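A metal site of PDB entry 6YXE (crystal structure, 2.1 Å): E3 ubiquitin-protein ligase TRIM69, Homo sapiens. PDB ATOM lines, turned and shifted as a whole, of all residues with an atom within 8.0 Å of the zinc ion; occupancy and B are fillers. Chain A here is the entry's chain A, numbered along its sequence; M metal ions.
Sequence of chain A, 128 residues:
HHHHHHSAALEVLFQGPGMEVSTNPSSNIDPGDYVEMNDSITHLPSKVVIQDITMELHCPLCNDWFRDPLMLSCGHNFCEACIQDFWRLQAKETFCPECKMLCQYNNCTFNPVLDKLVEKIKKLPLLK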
ATOM      1  N   LEU A  72      14.896  19.721 -17.423  1.00  0.00           N
ATOM      2  CA  LEU A  72      14.629  20.317 -16.119  1.00  0.00           C
ATOM      3  C   LEU A  72      13.133  20.505 -15.986  1.00  0.00           C
ATOM      4  O   LEU A  72      12.385  20.322 -16.970  1.00  0.00           O
ATOM      5  CB  LEU A  72      15.320  21.672 -15.963  1.00  0.00           C
ATOM      6  CG  LEU A  72      16.764  21.844 -16.418  1.00  0.00           C
ATOM      7  CD1 LEU A  72      17.269  23.206 -15.958  1.00  0.00           C
ATOM      8  CD2 LEU A  72      17.650  20.707 -15.952  1.00  0.00           C
ATOM      9  N   SER A  73      12.724  20.900 -14.787  1.00  0.00           N
ATOM     10  CA  SER A  73      11.313  21.032 -14.461  1.00  0.00           C
ATOM     11  C   SER A  73      10.575  22.024 -15.374  1.00  0.00           C
ATOM     12  O   SER A  73       9.370  21.904 -15.555  1.00  0.00           O
ATOM     13  CB  SER A  73      11.123  21.462 -12.986  1.00  0.00           C
ATOM     14  OG  SER A  73      12.189  21.000 -12.160  1.00  0.00           O
ATOM     15  N   CYS A  74      11.288  23.014 -15.901  1.00  0.00           N
ATOM     16  CA  CYS A  74      10.717  23.986 -16.817  1.00  0.00           C
ATOM     17  C   CYS A  74      10.523  23.451 -18.247  1.00  0.00           C
ATOM     18  O   CYS A  74       9.880  24.115 -19.011  1.00  0.00           O
ATOM     19  CB  CYS A  74      11.585  25.226 -16.876  1.00  0.00           C
ATOM     20  SG  CYS A  74      13.273  24.824 -17.373  1.00  0.00           S
ATOM     21  N   GLY A  75      11.094  22.308 -18.611  1.00  0.00           N
ATOM     22  CA  GLY A  75      10.996  21.770 -19.963  1.00  0.00           C
ATOM     23  C   GLY A  75      12.191  21.997 -20.864  1.00  0.00           C
ATOM     24  O   GLY A  75      12.263  21.396 -21.958  1.00  0.00           O
ATOM     25  N   HIS A  76      13.137  22.851 -20.435  1.00  0.00           N
ATOM     26  CA  HIS A  76      14.413  22.998 -21.136  1.00  0.00           C
ATOM     27  C   HIS A  76      15.366  21.815 -20.886  1.00  0.00           C
ATOM     28  O   HIS A  76      15.315  21.160 -19.855  1.00  0.00           O
ATOM     29  CB  HIS A  76      15.129  24.297 -20.778  1.00  0.00           C
ATOM     30  CG  HIS A  76      14.426  25.486 -21.299  1.00  0.00           C
ATOM     31  ND1 HIS A  76      13.826  26.424 -20.480  1.00  0.00           N
ATOM     32  CD2 HIS A  76      14.142  25.875 -22.577  1.00  0.00           C
ATOM     33  CE1 HIS A  76      13.210  27.318 -21.228  1.00  0.00           C
ATOM     34  NE2 HIS A  76      13.399  27.015 -22.498  1.00  0.00           N
ATOM     35  N   ASN A  77      16.211  21.596 -21.870  1.00  0.00           N
ATOM     36  CA  ASN A  77      17.114  20.457 -21.982  1.00  0.00           C
ATOM     37  C   ASN A  77      18.551  20.958 -22.091  1.00  0.00           C
ATOM     38  O   ASN A  77      18.805  21.973 -22.747  1.00  0.00           O
ATOM     39  CB  ASN A  77      16.810  19.634 -23.243  1.00  0.00           C
ATOM     40  CG  ASN A  77      15.431  18.990 -23.198  1.00  0.00           C
ATOM     41  OD1 ASN A  77      15.203  18.027 -22.462  1.00  0.00           O
ATOM     42  ND2 ASN A  77      14.490  19.570 -23.931  1.00  0.00           N
ATOM     43  N   PHE A  78      19.470  20.233 -21.458  1.00  0.00           N
ATOM     44  CA  PHE A  78      20.925  20.495 -21.505  1.00  0.00           C
ATOM     45  C   PHE A  78      21.644  19.165 -21.402  1.00  0.00           C
ATOM     46  O   PHE A  78      21.119  18.269 -20.731  1.00  0.00           O
ATOM     47  CB  PHE A  78      21.358  21.358 -20.309  1.00  0.00           C
ATOM     48  CG  PHE A  78      20.576  22.612 -20.196  1.00  0.00           C
ATOM     49  CD1 PHE A  78      20.986  23.757 -20.853  1.00  0.00           C
ATOM     50  CD2 PHE A  78      19.374  22.634 -19.497  1.00  0.00           C
ATOM     51  CE1 PHE A  78      20.211  24.915 -20.819  1.00  0.00           C
ATOM     52  CE2 PHE A  78      18.601  23.777 -19.454  1.00  0.00           C
ATOM     53  CZ  PHE A  78      19.029  24.913 -20.119  1.00  0.00           C
ATOM     54  N   PHE A  95      18.985  26.964 -10.872  1.00  0.00           N
ATOM     55  CA  PHE A  95      18.070  27.562 -11.832  1.00  0.00           C
ATOM     56  C   PHE A  95      18.403  27.171 -13.289  1.00  0.00           C
ATOM     57  O   PHE A  95      19.517  26.746 -13.613  1.00  0.00           O
ATOM     58  CB  PHE A  95      18.029  29.083 -11.657  1.00  0.00           C
ATOM     59  CG  PHE A  95      19.304  29.792 -11.999  1.00  0.00           C
ATOM     60  CD1 PHE A  95      19.573  30.199 -13.301  1.00  0.00           C
ATOM     61  CD2 PHE A  95      20.237  30.097 -11.002  1.00  0.00           C
ATOM     62  CE1 PHE A  95      20.756  30.842 -13.625  1.00  0.00           C
ATOM     63  CE2 PHE A  95      21.400  30.786 -11.316  1.00  0.00           C
ATOM     64  CZ  PHE A  95      21.663  31.142 -12.643  1.00  0.00           C
ATOM     65  N   CYS A  96      17.413  27.318 -14.152  1.00  0.00           N
ATOM     66  CA  CYS A  96      17.585  27.056 -15.574  1.00  0.00           C
ATOM     67  C   CYS A  96      18.340  28.221 -16.209  1.00  0.00           C
ATOM     68  O   CYS A  96      17.899  29.350 -16.120  1.00  0.00           O
ATOM     69  CB  CYS A  96      16.242  26.895 -16.252  1.00  0.00           C
ATOM     70  SG  CYS A  96      16.347  26.671 -18.008  1.00  0.00           S
ATOM     71  N   PRO A  97      19.482  27.950 -16.851  1.00  0.00           N
ATOM     72  CA  PRO A  97      20.206  28.996 -17.574  1.00  0.00           C
ATOM     73  C   PRO A  97      19.401  29.727 -18.646  1.00  0.00           C
ATOM     74  O   PRO A  97      19.739  30.844 -18.941  1.00  0.00           O
ATOM     75  CB  PRO A  97      21.358  28.251 -18.268  1.00  0.00           C
ATOM     76  CG  PRO A  97      21.320  26.872 -17.782  1.00  0.00           C
ATOM     77  CD  PRO A  97      20.106  26.617 -16.978  1.00  0.00           C
ATOM     78  N   GLU A  98      18.400  29.088 -19.258  1.00  0.00           N
ATOM     79  CA  GLU A  98      17.577  29.740 -20.299  1.00  0.00           C
ATOM     80  C   GLU A  98      16.505  30.642 -19.740  1.00  0.00           C
ATOM     81  O   GLU A  98      16.472  31.813 -20.044  1.00  0.00           O
ATOM     82  CB  GLU A  98      16.916  28.717 -21.244  1.00  0.00           C
ATOM     83  CG  GLU A  98      17.936  27.979 -22.093  1.00  0.00           C
ATOM     84  CD  GLU A  98      18.445  28.840 -23.249  1.00  0.00           C
ATOM     85  OE1 GLU A  98      17.810  28.796 -24.323  1.00  0.00           O
ATOM     86  OE2 GLU A  98      19.470  29.545 -23.096  1.00  0.00           O
ATOM     87  N   CYS A  99      15.604  30.074 -18.941  1.00  0.00           N
ATOM     88  CA  CYS A  99      14.427  30.803 -18.447  1.00  0.00           C
ATOM     89  C   CYS A  99      14.556  31.293 -17.013  1.00  0.00           C
ATOM     90  O   CYS A  99      13.687  31.992 -16.549  1.00  0.00           O
ATOM     91  CB  CYS A  99      13.162  29.948 -18.595  1.00  0.00           C
ATOM     92  SG  CYS A  99      13.061  28.481 -17.537  1.00  0.00           S
ATOM     93  N   LYS A 100      15.629  30.928 -16.329  1.00  0.00           N
ATOM     94  CA  LYS A 100      15.913  31.406 -14.960  1.00  0.00           C
ATOM     95  C   LYS A 100      14.997  30.863 -13.887  1.00  0.00           C
ATOM     96  O   LYS A 100      15.131  31.233 -12.758  1.00  0.00           O
ATOM     97  CB  LYS A 100      15.945  32.949 -14.882  1.00  0.00           C
ATOM     98  CG  LYS A 100      16.854  33.618 -15.904  1.00  0.00           C
ATOM     99  CD  LYS A 100      18.307  33.225 -15.666  1.00  0.00           C
ATOM    100  CE  LYS A 100      19.289  34.134 -16.388  1.00  0.00           C
ATOM    101  NZ  LYS A 100      19.377  33.774 -17.833  1.00  0.00           N
ATOM    102  N   MET A 101      14.092  29.941 -14.223  1.00  0.00           N
ATOM    103  CA  MET A 101      13.205  29.358 -13.219  1.00  0.00           C
ATOM    104  C   MET A 101      13.966  28.428 -12.266  1.00  0.00           C
ATOM    105  O   MET A 101      14.908  27.720 -12.677  1.00  0.00           O
ATOM    106  CB  MET A 101      12.067  28.620 -13.926  1.00  0.00           C
ATOM    107  CG  MET A 101      11.222  27.706 -13.068  1.00  0.00           C
ATOM    108  SD  MET A 101       9.782  27.144 -14.005  1.00  0.00           S
ATOM    109  CE  MET A 101       9.893  25.379 -13.661  1.00  0.00           C
ATOM    110  N   LEU A 102      13.530  28.399 -11.019  1.00  0.00           N
ATOM    111  CA  LEU A 102      14.161  27.595  -9.995  1.00  0.00           C
ATOM    112  C   LEU A 102      13.681  26.143 -10.144  1.00  0.00           C
ATOM    113  O   LEU A 102      12.540  25.780  -9.857  1.00  0.00           O
ATOM    114  CB  LEU A 102      13.916  28.117  -8.572  1.00  0.00           C
ATOM    115  CG  LEU A 102      15.085  27.702  -7.642  1.00  0.00           C
ATOM    116  CD1 LEU A 102      16.230  28.695  -7.746  1.00  0.00           C
ATOM    117  CD2 LEU A 102      14.670  27.559  -6.188  1.00  0.00           C
ATOM    118  N   CYS A 103      14.594  25.324 -10.621  1.00  0.00           N
ATOM    119  CA  CYS A 103      14.316  23.903 -10.782  1.00  0.00           C
ATOM    120  C   CYS A 103      14.873  23.245  -9.543  1.00  0.00           C
ATOM    121  O   CYS A 103      15.796  23.764  -8.925  1.00  0.00           O
ATOM    122  CB  CYS A 103      14.976  23.419 -12.078  1.00  0.00           C
ATOM    123  SG  CYS A 103      14.377  24.347 -13.513  1.00  0.00           S
HETATM  124 ZN    ZN M   1      14.089  26.610 -18.490  1.00  0.00          ZN
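Four residues have an atom within 4 Å of the zinc ion: Cys 74, His 76, Cys 96 and Cys 99.
The side-chain sulfur (SG) of Cys 96 sits close to the backbone NH (N) of Glu 98 (3.4 Å). The backbone carbonyl oxygen (O) of Met 101 sits at hydrogen-bond distance from the backbone NH (N) of Cys 96, at 2.9 Å. The side-chain sulfur (SG) of Cys 99 sits close to the backbone NH (N) of Met 101, 3.8 Å away.
The zinc ion is bound by ND1 of His 76 (2.0 Å), SG of Cys 74 (2.3 Å), SG of Cys 96 (2.3 Å) and SG of Cys 99 (2.3 Å).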
